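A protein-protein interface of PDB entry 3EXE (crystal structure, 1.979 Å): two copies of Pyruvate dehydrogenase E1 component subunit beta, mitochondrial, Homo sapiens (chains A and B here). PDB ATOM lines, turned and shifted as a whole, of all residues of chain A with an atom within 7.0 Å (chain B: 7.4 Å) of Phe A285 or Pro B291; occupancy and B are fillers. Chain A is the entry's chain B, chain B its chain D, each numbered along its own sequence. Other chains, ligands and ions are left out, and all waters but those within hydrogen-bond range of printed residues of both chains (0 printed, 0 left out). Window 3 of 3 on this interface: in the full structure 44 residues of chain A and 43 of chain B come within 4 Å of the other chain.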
ATOM      1  N   GLU A 250      16.621 -12.546  22.986  1.00  0.00           N
ATOM      2  CA  GLU A 250      16.984 -13.903  23.351  1.00  0.00           C
ATOM      3  C   GLU A 250      16.389 -14.925  22.431  1.00  0.00           C
ATOM      4  O   GLU A 250      17.085 -15.847  22.036  1.00  0.00           O
ATOM      5  CB  GLU A 250      16.688 -14.178  24.836  1.00  0.00           C
ATOM      6  CG  GLU A 250      17.745 -13.448  25.642  1.00  0.00           C
ATOM      7  CD  GLU A 250      17.470 -13.351  27.159  1.00  0.00           C
ATOM      8  OE1 GLU A 250      16.331 -13.678  27.581  1.00  0.00           O
ATOM      9  OE2 GLU A 250      18.440 -12.945  27.892  1.00  0.00           O
ATOM     10  N   VAL A 253      18.270 -14.873  19.129  1.00  0.00           N
ATOM     11  CA  VAL A 253      19.609 -15.464  19.150  1.00  0.00           C
ATOM     12  C   VAL A 253      19.530 -16.963  19.321  1.00  0.00           C
ATOM     13  O   VAL A 253      20.445 -17.704  18.922  1.00  0.00           O
ATOM     14  CB  VAL A 253      20.433 -14.868  20.323  1.00  0.00           C
ATOM     15  CG1 VAL A 253      21.652 -15.726  20.600  1.00  0.00           C
ATOM     16  CG2 VAL A 253      20.784 -13.405  20.065  1.00  0.00           C
ATOM     17  N   MET A 254      18.484 -17.436  20.001  1.00  0.00           N
ATOM     18  CA  MET A 254      18.307 -18.885  20.082  1.00  0.00           C
ATOM     19  C   MET A 254      18.052 -19.518  18.714  1.00  0.00           C
ATOM     20  O   MET A 254      18.351 -20.690  18.507  1.00  0.00           O
ATOM     21  CB  MET A 254      17.208 -19.239  21.060  1.00  0.00           C
ATOM     22  CG  MET A 254      17.618 -19.057  22.508  1.00  0.00           C
ATOM     23  SD  MET A 254      16.116 -19.219  23.503  1.00  0.00           S
ATOM     24  CE  MET A 254      16.776 -19.024  25.134  1.00  0.00           C
ATOM     25  N   CYS A 276      24.713  -7.178  25.767  1.00  0.00           N
ATOM     26  CA  CYS A 276      25.726  -8.248  25.828  1.00  0.00           C
ATOM     27  C   CYS A 276      25.793  -8.919  27.196  1.00  0.00           C
ATOM     28  O   CYS A 276      25.917 -10.142  27.298  1.00  0.00           O
ATOM     29  CB  CYS A 276      27.085  -7.640  25.467  1.00  0.00           C
ATOM     30  SG  CYS A 276      27.217  -7.293  23.660  1.00  0.00           S
ATOM     31  N   ARG A 278      23.369  -8.979  29.502  1.00  0.00           N
ATOM     32  CA  ARG A 278      22.143  -9.781  29.630  1.00  0.00           C
ATOM     33  C   ARG A 278      22.183 -11.062  28.799  1.00  0.00           C
ATOM     34  O   ARG A 278      21.733 -12.124  29.242  1.00  0.00           O
ATOM     35  CB  ARG A 278      20.912  -8.967  29.185  1.00  0.00           C
ATOM     36  CG  ARG A 278      20.669  -7.718  30.028  1.00  0.00           C
ATOM     37  CD  ARG A 278      20.011  -8.095  31.313  1.00  0.00           C
ATOM     38  NE  ARG A 278      18.572  -8.108  31.088  1.00  0.00           N
ATOM     39  CZ  ARG A 278      17.881  -6.976  30.981  1.00  0.00           C
ATOM     40  NH1 ARG A 278      18.496  -5.778  31.146  1.00  0.00           N
ATOM     41  NH2 ARG A 278      16.609  -7.045  30.735  1.00  0.00           N
ATOM     42  N   ILE A 279      22.651 -10.986  27.560  1.00  0.00           N
ATOM     43  CA  ILE A 279      22.728 -12.223  26.776  1.00  0.00           C
ATOM     44  C   ILE A 279      23.639 -13.269  27.456  1.00  0.00           C
ATOM     45  O   ILE A 279      23.308 -14.472  27.523  1.00  0.00           O
ATOM     46  CB  ILE A 279      23.175 -11.944  25.322  1.00  0.00           C
ATOM     47  CG1 ILE A 279      21.949 -11.554  24.459  1.00  0.00           C
ATOM     48  CG2 ILE A 279      23.815 -13.152  24.714  1.00  0.00           C
ATOM     49  CD1 ILE A 279      21.046 -12.702  24.068  1.00  0.00           C
ATOM     50  N   MET A 280      24.774 -12.824  27.968  1.00  0.00           N
ATOM     51  CA  MET A 280      25.662 -13.707  28.720  1.00  0.00           C
ATOM     52  C   MET A 280      25.054 -14.254  30.044  1.00  0.00           C
ATOM     53  O   MET A 280      25.199 -15.436  30.358  1.00  0.00           O
ATOM     54  CB  MET A 280      27.039 -13.066  28.927  1.00  0.00           C
ATOM     55  CG  MET A 280      27.953 -14.036  29.733  1.00  0.00           C
ATOM     56  SD  MET A 280      29.696 -13.883  29.364  1.00  0.00           S
ATOM     57  CE  MET A 280      29.930 -12.090  29.490  1.00  0.00           C
ATOM     58  N   GLU A 281      24.316 -13.434  30.781  1.00  0.00           N
ATOM     59  CA  GLU A 281      23.681 -13.928  31.985  1.00  0.00           C
ATOM     60  C   GLU A 281      22.462 -14.820  31.735  1.00  0.00           C
ATOM     61  O   GLU A 281      22.008 -15.453  32.671  1.00  0.00           O
ATOM     62  CB  GLU A 281      23.223 -12.775  32.889  1.00  0.00           C
ATOM     63  CG  GLU A 281      24.378 -12.036  33.552  1.00  0.00           C
ATOM     64  CD  GLU A 281      23.860 -10.768  34.270  1.00  0.00           C
ATOM     65  OE1 GLU A 281      22.830 -10.195  33.803  1.00  0.00           O
ATOM     66  OE2 GLU A 281      24.426 -10.405  35.324  1.00  0.00           O
ATOM     67  N   GLY A 282      21.917 -14.821  30.506  1.00  0.00           N
ATOM     68  CA  GLY A 282      20.586 -15.369  30.278  1.00  0.00           C
ATOM     69  C   GLY A 282      20.571 -16.700  29.556  1.00  0.00           C
ATOM     70  O   GLY A 282      21.596 -17.326  29.391  1.00  0.00           O
ATOM     71  N   PRO A 283      19.378 -17.153  29.158  1.00  0.00           N
ATOM     72  CA  PRO A 283      19.182 -18.491  28.606  1.00  0.00           C
ATOM     73  C   PRO A 283      19.736 -18.680  27.175  1.00  0.00           C
ATOM     74  O   PRO A 283      19.860 -19.797  26.691  1.00  0.00           O
ATOM     75  CB  PRO A 283      17.653 -18.658  28.664  1.00  0.00           C
ATOM     76  CG  PRO A 283      17.119 -17.212  28.506  1.00  0.00           C
ATOM     77  CD  PRO A 283      18.096 -16.450  29.397  1.00  0.00           C
ATOM     78  N   ALA A 284      20.074 -17.597  26.489  1.00  0.00           N
ATOM     79  CA  ALA A 284      20.492 -17.706  25.104  1.00  0.00           C
ATOM     80  C   ALA A 284      22.007 -17.875  25.038  1.00  0.00           C
ATOM     81  O   ALA A 284      22.542 -18.161  23.967  1.00  0.00           O
ATOM     82  CB  ALA A 284      20.081 -16.397  24.319  1.00  0.00           C
ATOM     83  N   PHE A 285      22.712 -17.677  26.154  1.00  0.00           N
ATOM     84  CA  PHE A 285      24.197 -17.688  26.085  1.00  0.00           C
ATOM     85  C   PHE A 285      24.707 -18.975  25.414  1.00  0.00           C
ATOM     86  O   PHE A 285      25.550 -18.932  24.507  1.00  0.00           O
ATOM     87  CB  PHE A 285      24.815 -17.558  27.488  1.00  0.00           C
ATOM     88  CG  PHE A 285      26.335 -17.506  27.488  1.00  0.00           C
ATOM     89  CD1 PHE A 285      26.995 -16.482  26.834  1.00  0.00           C
ATOM     90  CD2 PHE A 285      27.089 -18.490  28.129  1.00  0.00           C
ATOM     91  CE1 PHE A 285      28.377 -16.428  26.836  1.00  0.00           C
ATOM     92  CE2 PHE A 285      28.489 -18.450  28.125  1.00  0.00           C
ATOM     93  CZ  PHE A 285      29.125 -17.387  27.486  1.00  0.00           C
ATOM     94  N   ASN A 286      24.237 -20.135  25.885  1.00  0.00           N
ATOM     95  CA  ASN A 286      24.689 -21.386  25.290  1.00  0.00           C
ATOM     96  C   ASN A 286      24.339 -21.527  23.807  1.00  0.00           C
ATOM     97  O   ASN A 286      24.883 -22.386  23.119  1.00  0.00           O
ATOM     98  CB  ASN A 286      24.130 -22.587  26.043  1.00  0.00           C
ATOM     99  CG  ASN A 286      24.819 -22.779  27.372  1.00  0.00           C
ATOM    100  OD1 ASN A 286      25.964 -22.341  27.555  1.00  0.00           O
ATOM    101  ND2 ASN A 286      24.140 -23.427  28.299  1.00  0.00           N
ATOM    102  N   PHE A 287      23.425 -20.717  23.328  1.00  0.00           N
ATOM    103  CA  PHE A 287      23.084 -20.752  21.900  1.00  0.00           C
ATOM    104  C   PHE A 287      24.047 -19.948  21.009  1.00  0.00           C
ATOM    105  O   PHE A 287      24.044 -20.077  19.773  1.00  0.00           O
ATOM    106  CB  PHE A 287      21.665 -20.262  21.697  1.00  0.00           C
ATOM    107  CG  PHE A 287      20.653 -21.234  22.156  1.00  0.00           C
ATOM    108  CD1 PHE A 287      19.963 -21.988  21.248  1.00  0.00           C
ATOM    109  CD2 PHE A 287      20.384 -21.381  23.509  1.00  0.00           C
ATOM    110  CE1 PHE A 287      19.026 -22.900  21.667  1.00  0.00           C
ATOM    111  CE2 PHE A 287      19.417 -22.283  23.955  1.00  0.00           C
ATOM    112  CZ  PHE A 287      18.741 -23.052  23.029  1.00  0.00           C
ATOM    113  N   LEU A 288      24.886 -19.150  21.638  1.00  0.00           N
ATOM    114  CA  LEU A 288      25.833 -18.338  20.907  1.00  0.00           C
ATOM    115  C   LEU A 288      26.998 -19.148  20.323  1.00  0.00           C
ATOM    116  O   LEU A 288      27.737 -19.775  21.076  1.00  0.00           O
ATOM    117  CB  LEU A 288      26.409 -17.242  21.828  1.00  0.00           C
ATOM    118  CG  LEU A 288      25.615 -15.955  22.070  1.00  0.00           C
ATOM    119  CD1 LEU A 288      26.425 -15.051  22.969  1.00  0.00           C
ATOM    120  CD2 LEU A 288      25.375 -15.208  20.724  1.00  0.00           C
ATOM    121  N   ASP A 289      27.184 -19.083  19.006  1.00  0.00           N
ATOM    122  CA  ASP A 289      28.259 -19.838  18.334  1.00  0.00           C
ATOM    123  C   ASP A 289      29.457 -18.900  18.120  1.00  0.00           C
ATOM    124  O   ASP A 289      30.494 -19.303  17.591  1.00  0.00           O
ATOM    125  CB  ASP A 289      27.820 -20.352  16.965  1.00  0.00           C
ATOM    126  CG  ASP A 289      26.844 -21.536  17.034  1.00  0.00           C
ATOM    127  OD1 ASP A 289      26.695 -22.163  18.108  1.00  0.00           O
ATOM    128  OD2 ASP A 289      26.221 -21.840  15.973  1.00  0.00           O
ATOM    129  N   ALA A 290      29.310 -17.652  18.531  1.00  0.00           N
ATOM    130  CA  ALA A 290      30.422 -16.690  18.491  1.00  0.00           C
ATOM    131  C   ALA A 290      30.129 -15.616  19.511  1.00  0.00           C
ATOM    132  O   ALA A 290      28.974 -15.419  19.879  1.00  0.00           O
ATOM    133  CB  ALA A 290      30.552 -16.033  17.089  1.00  0.00           C
ATOM    134  N   PRO A 291      31.157 -14.875  19.930  1.00  0.00           N
ATOM    135  CA  PRO A 291      30.823 -13.834  20.899  1.00  0.00           C
ATOM    136  C   PRO A 291      29.884 -12.759  20.295  1.00  0.00           C
ATOM    137  O   PRO A 291      29.923 -12.458  19.064  1.00  0.00           O
ATOM    138  CB  PRO A 291      32.179 -13.215  21.275  1.00  0.00           C
ATOM    139  CG  PRO A 291      33.155 -13.696  20.233  1.00  0.00           C
ATOM    140  CD  PRO A 291      32.554 -14.840  19.466  1.00  0.00           C
ATOM    141  N   ILE B 207      38.270 -18.547  40.621  1.00  0.00           N
ATOM    142  CA  ILE B 207      37.350 -17.565  40.061  1.00  0.00           C
ATOM    143  C   ILE B 207      37.931 -16.182  40.267  1.00  0.00           C
ATOM    144  O   ILE B 207      38.539 -15.877  41.328  1.00  0.00           O
ATOM    145  CB  ILE B 207      35.926 -17.626  40.755  1.00  0.00           C
ATOM    146  CG1 ILE B 207      34.863 -16.715  40.061  1.00  0.00           C
ATOM    147  CG2 ILE B 207      36.067 -17.317  42.275  1.00  0.00           C
ATOM    148  CD1 ILE B 207      33.462 -17.210  40.345  1.00  0.00           C
ATOM    149  N   ASN B 257      39.170 -19.044  34.664  1.00  0.00           N
ATOM    150  CA  ASN B 257      38.061 -19.479  33.787  1.00  0.00           C
ATOM    151  C   ASN B 257      36.651 -19.033  34.216  1.00  0.00           C
ATOM    152  O   ASN B 257      35.616 -19.474  33.654  1.00  0.00           O
ATOM    153  CB  ASN B 257      38.129 -21.026  33.526  1.00  0.00           C
ATOM    154  CG  ASN B 257      39.546 -21.509  33.222  1.00  0.00           C
ATOM    155  OD1 ASN B 257      40.118 -22.310  33.975  1.00  0.00           O
ATOM    156  ND2 ASN B 257      40.117 -21.048  32.101  1.00  0.00           N
ATOM    157  N   HIS B 258      36.591 -18.147  35.219  1.00  0.00           N
ATOM    158  CA  HIS B 258      35.305 -17.795  35.808  1.00  0.00           C
ATOM    159  C   HIS B 258      35.383 -16.350  36.226  1.00  0.00           C
ATOM    160  O   HIS B 258      36.466 -15.901  36.647  1.00  0.00           O
ATOM    161  CB  HIS B 258      34.957 -18.699  37.020  1.00  0.00           C
ATOM    162  CG  HIS B 258      34.795 -20.158  36.668  1.00  0.00           C
ATOM    163  ND1 HIS B 258      35.865 -21.022  36.591  1.00  0.00           N
ATOM    164  CD2 HIS B 258      33.697 -20.896  36.380  1.00  0.00           C
ATOM    165  CE1 HIS B 258      35.433 -22.236  36.287  1.00  0.00           C
ATOM    166  NE2 HIS B 258      34.125 -22.182  36.138  1.00  0.00           N
ATOM    167  N   LEU B 259      34.245 -15.641  36.117  1.00  0.00           N
ATOM    168  CA  LEU B 259      34.201 -14.207  36.419  1.00  0.00           C
ATOM    169  C   LEU B 259      32.890 -13.818  37.065  1.00  0.00           C
ATOM    170  O   LEU B 259      31.788 -14.170  36.548  1.00  0.00           O
ATOM    171  CB  LEU B 259      34.421 -13.344  35.127  1.00  0.00           C
ATOM    172  CG  LEU B 259      34.342 -11.799  35.304  1.00  0.00           C
ATOM    173  CD1 LEU B 259      35.438 -11.282  36.261  1.00  0.00           C
ATOM    174  CD2 LEU B 259      34.497 -11.087  33.997  1.00  0.00           C
ATOM    175  N   VAL B 260      32.994 -13.127  38.202  1.00  0.00           N
ATOM    176  CA  VAL B 260      31.871 -12.438  38.814  1.00  0.00           C
ATOM    177  C   VAL B 260      32.273 -10.950  39.022  1.00  0.00           C
ATOM    178  O   VAL B 260      33.358 -10.677  39.530  1.00  0.00           O
ATOM    179  CB  VAL B 260      31.452 -13.088  40.164  1.00  0.00           C
ATOM    180  CG1 VAL B 260      30.283 -12.256  40.911  1.00  0.00           C
ATOM    181  CG2 VAL B 260      31.034 -14.534  39.908  1.00  0.00           C
ATOM    182  N   CYS B 276      31.585  -7.178  31.548  1.00  0.00           N
ATOM    183  CA  CYS B 276      31.006  -8.374  30.922  1.00  0.00           C
ATOM    184  C   CYS B 276      31.077  -8.274  29.393  1.00  0.00           C
ATOM    185  O   CYS B 276      31.443  -9.242  28.720  1.00  0.00           O
ATOM    186  CB  CYS B 276      29.538  -8.612  31.437  1.00  0.00           C
ATOM    187  SG  CYS B 276      29.662  -9.311  33.128  1.00  0.00           S
ATOM    188  N   MET B 280      33.529 -10.597  26.901  1.00  0.00           N
ATOM    189  CA  MET B 280      33.047 -11.320  25.705  1.00  0.00           C
ATOM    190  C   MET B 280      33.663 -10.907  24.345  1.00  0.00           C
ATOM    191  O   MET B 280      33.877 -11.751  23.488  1.00  0.00           O
ATOM    192  CB  MET B 280      31.517 -11.313  25.647  1.00  0.00           C
ATOM    193  CG  MET B 280      30.888 -12.014  24.385  1.00  0.00           C
ATOM    194  SD  MET B 280      29.249 -12.712  24.661  1.00  0.00           S
ATOM    195  CE  MET B 280      28.306 -11.397  25.464  1.00  0.00           C
ATOM    196  N   PHE B 285      37.464 -14.485  26.268  1.00  0.00           N
ATOM    197  CA  PHE B 285      36.117 -15.080  26.196  1.00  0.00           C
ATOM    198  C   PHE B 285      36.219 -16.607  26.109  1.00  0.00           C
ATOM    199  O   PHE B 285      35.504 -17.326  26.825  1.00  0.00           O
ATOM    200  CB  PHE B 285      35.316 -14.549  25.002  1.00  0.00           C
ATOM    201  CG  PHE B 285      33.902 -15.137  24.845  1.00  0.00           C
ATOM    202  CD1 PHE B 285      32.918 -14.899  25.812  1.00  0.00           C
ATOM    203  CD2 PHE B 285      33.547 -15.860  23.684  1.00  0.00           C
ATOM    204  CE1 PHE B 285      31.604 -15.358  25.657  1.00  0.00           C
ATOM    205  CE2 PHE B 285      32.200 -16.337  23.501  1.00  0.00           C
ATOM    206  CZ  PHE B 285      31.229 -16.094  24.498  1.00  0.00           C
ATOM    207  N   LEU B 288      36.579 -18.763  29.320  1.00  0.00           N
ATOM    208  CA  LEU B 288      35.462 -18.889  30.273  1.00  0.00           C
ATOM    209  C   LEU B 288      34.925 -20.321  30.308  1.00  0.00           C
ATOM    210  O   LEU B 288      34.666 -20.902  29.288  1.00  0.00           O
ATOM    211  CB  LEU B 288      34.310 -17.931  29.925  1.00  0.00           C
ATOM    212  CG  LEU B 288      34.542 -16.462  30.254  1.00  0.00           C
ATOM    213  CD1 LEU B 288      33.414 -15.585  29.685  1.00  0.00           C
ATOM    214  CD2 LEU B 288      34.676 -16.216  31.794  1.00  0.00           C
ATOM    215  N   ASP B 289      34.792 -20.893  31.490  1.00  0.00           N
ATOM    216  CA  ASP B 289      34.144 -22.186  31.631  1.00  0.00           C
ATOM    217  C   ASP B 289      32.693 -21.999  32.102  1.00  0.00           C
ATOM    218  O   ASP B 289      31.947 -22.964  32.229  1.00  0.00           O
ATOM    219  CB  ASP B 289      34.904 -23.040  32.655  1.00  0.00           C
ATOM    220  CG  ASP B 289      36.103 -23.750  32.037  1.00  0.00           C
ATOM    221  OD1 ASP B 289      36.278 -23.650  30.796  1.00  0.00           O
ATOM    222  OD2 ASP B 289      36.836 -24.446  32.776  1.00  0.00           O
ATOM    223  N   ALA B 290      32.328 -20.757  32.409  1.00  0.00           N
ATOM    224  CA  ALA B 290      30.930 -20.387  32.709  1.00  0.00           C
ATOM    225  C   ALA B 290      30.698 -18.965  32.307  1.00  0.00           C
ATOM    226  O   ALA B 290      31.647 -18.209  32.171  1.00  0.00           O
ATOM    227  CB  ALA B 290      30.580 -20.572  34.200  1.00  0.00           C
ATOM    228  N   PRO B 291      29.424 -18.584  32.124  1.00  0.00           N
ATOM    229  CA  PRO B 291      29.068 -17.184  31.862  1.00  0.00           C
ATOM    230  C   PRO B 291      29.585 -16.234  32.978  1.00  0.00           C
ATOM    231  O   PRO B 291      29.538 -16.570  34.174  1.00  0.00           O
ATOM    232  CB  PRO B 291      27.517 -17.175  31.867  1.00  0.00           C
ATOM    233  CG  PRO B 291      27.036 -18.605  32.179  1.00  0.00           C
ATOM    234  CD  PRO B 291      28.271 -19.512  32.102  1.00  0.00           C
ATOM    235  N   ALA B 292      30.056 -15.059  32.587  1.00  0.00           N
ATOM    236  CA  ALA B 292      30.354 -14.001  33.576  1.00  0.00           C
ATOM    237  C   ALA B 292      29.020 -13.494  34.111  1.00  0.00           C
ATOM    238  O   ALA B 292      28.056 -13.361  33.352  1.00  0.00           O
ATOM    239  CB  ALA B 292      31.153 -12.857  32.929  1.00  0.00           C
ATOM    240  N   VAL B 293      28.931 -13.232  35.415  1.00  0.00           N
ATOM    241  CA  VAL B 293      27.659 -12.741  35.954  1.00  0.00           C
ATOM    242  C   VAL B 293      27.913 -11.580  36.898  1.00  0.00           C
ATOM    243  O   VAL B 293      29.018 -11.386  37.387  1.00  0.00           O
ATOM    244  CB  VAL B 293      26.846 -13.848  36.671  1.00  0.00           C
ATOM    245  CG1 VAL B 293      26.426 -14.916  35.691  1.00  0.00           C
ATOM    246  CG2 VAL B 293      27.632 -14.430  37.929  1.00  0.00           C
ATOM    247  N   ARG B 294      26.854 -10.822  37.187  1.00  0.00           N
ATOM    248  CA  ARG B 294      27.007  -9.568  37.911  1.00  0.00           C
ATOM    249  C   ARG B 294      26.200  -9.539  39.223  1.00  0.00           C
ATOM    250  O   ARG B 294      25.034  -9.951  39.262  1.00  0.00           O
ATOM    251  CB  ARG B 294      26.540  -8.393  37.008  1.00  0.00           C
ATOM    252  CG  ARG B 294      27.203  -8.309  35.591  1.00  0.00           C
ATOM    253  CD  ARG B 294      26.487  -7.173  34.838  1.00  0.00           C
ATOM    254  NE  ARG B 294      25.168  -7.616  34.335  1.00  0.00           N
ATOM    255  CZ  ARG B 294      24.271  -6.818  33.725  1.00  0.00           C
ATOM    256  NH1 ARG B 294      24.499  -5.521  33.631  1.00  0.00           N
ATOM    257  NH2 ARG B 294      23.123  -7.289  33.250  1.00  0.00           N
ATOM    258  N   ALA B 322      26.379 -15.902  44.028  1.00  0.00           N
ATOM    259  CA  ALA B 322      26.786 -15.753  42.624  1.00  0.00           C
ATOM    260  C   ALA B 322      28.010 -16.594  42.274  1.00  0.00           C
ATOM    261  O   ALA B 322      28.047 -17.234  41.227  1.00  0.00           O
ATOM    262  CB  ALA B 322      27.084 -14.263  42.306  1.00  0.00           C
ATOM    263  N   LYS B 325      27.032 -20.247  42.221  1.00  0.00           N
ATOM    264  CA  LYS B 325      26.302 -20.497  40.970  1.00  0.00           C
ATOM    265  C   LYS B 325      27.293 -20.673  39.799  1.00  0.00           C
ATOM    266  O   LYS B 325      27.136 -21.571  38.947  1.00  0.00           O
ATOM    267  CB  LYS B 325      25.351 -19.357  40.675  1.00  0.00           C
ATOM    268  CG  LYS B 325      24.095 -19.437  41.444  1.00  0.00           C
ATOM    269  CD  LYS B 325      23.230 -20.599  40.887  1.00  0.00           C
ATOM    270  CE  LYS B 325      21.918 -20.712  41.655  1.00  0.00           C
ATOM    271  NZ  LYS B 325      20.919 -21.486  40.906  1.00  0.00           N
ATOM    272  N   THR B 326      28.317 -19.821  39.771  1.00  0.00           N
ATOM    273  CA  THR B 326      29.248 -19.742  38.632  1.00  0.00           C
ATOM    274  C   THR B 326      30.112 -20.988  38.616  1.00  0.00           C
ATOM    275  O   THR B 326      30.352 -21.545  37.564  1.00  0.00           O
ATOM    276  CB  THR B 326      30.140 -18.470  38.726  1.00  0.00           C
ATOM    277  OG1 THR B 326      29.305 -17.307  38.595  1.00  0.00           O
ATOM    278  CG2 THR B 326      31.172 -18.491  37.651  1.00  0.00           C
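Among the printed residues, merely in contact across the chains: Pro A291 with Met B280, Cys A276 with Met B280, Met A280 with Pro B291, Met A280 with Cys B276, Phe A285 with Phe B285, Arg A278 with Arg B294, Pro A291 with Phe B285, Glu A281 with Ala B292 and Phe A285 with Pro B291.
Of the 18 printed residues of chain A, 6 touch a printed residue of chain B. Printed residues of chain A that touch a printed residue of chain B: Cys A276, Arg A278, Met A280, Glu A281, Phe A285 and Pro A291. Among the printed residues, 11 pairs touch across the chains. Among the printed residues, Asp or Glu carboxylates within 4 Å of a Lys or Arg side-chain nitrogen of the other chain: Glu A281 with Arg B294 (3.0 Å).
Cys A276 touches Met B280, and with the chains exchanged Met A280 touches Cys B276. Met A280 touches Pro B291, and with the chains exchanged Pro A291 touches Met B280. Phe B285 touches its own counterpart, Phe A285. Phe A285 touches Pro B291, and with the chains exchanged Pro A291 touches Phe B285.
Printed residues of chain B within 4 Å of Phe A285: Phe B285 (3.6 Å) and Pro B291 (3.99 Å). Printed residues of chain A within 4 Å of Pro B291: Met A280 and Phe A285. Of the printed residues of chain A, Arg B294 touches Arg A278 (3.8 Å) and Glu A281 (3.0 Å). Printed residues of chain A within 4 Å of Phe B285: Phe A285 and Pro A291. Of the printed residues of chain A, Met B280 touches Cys A276 and Pro A291. Of the printed residues of chain B, Arg A278 touches Arg B294. The nearest printed residue of chain B that does not touch Phe A285 is Met B280 (4.4 Å). The nearest printed residue of chain B that does not touch Cys A276 is Cys B276 (5.6 Å).
The side-chain sulfur of Met A280 lies within hydrogen-bond range of the backbone NH of Ala B292, 3.4 Å away. OE1 of Glu A281 lies within salt-bridge range of NH2 of Arg B294 (3.0 Å).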
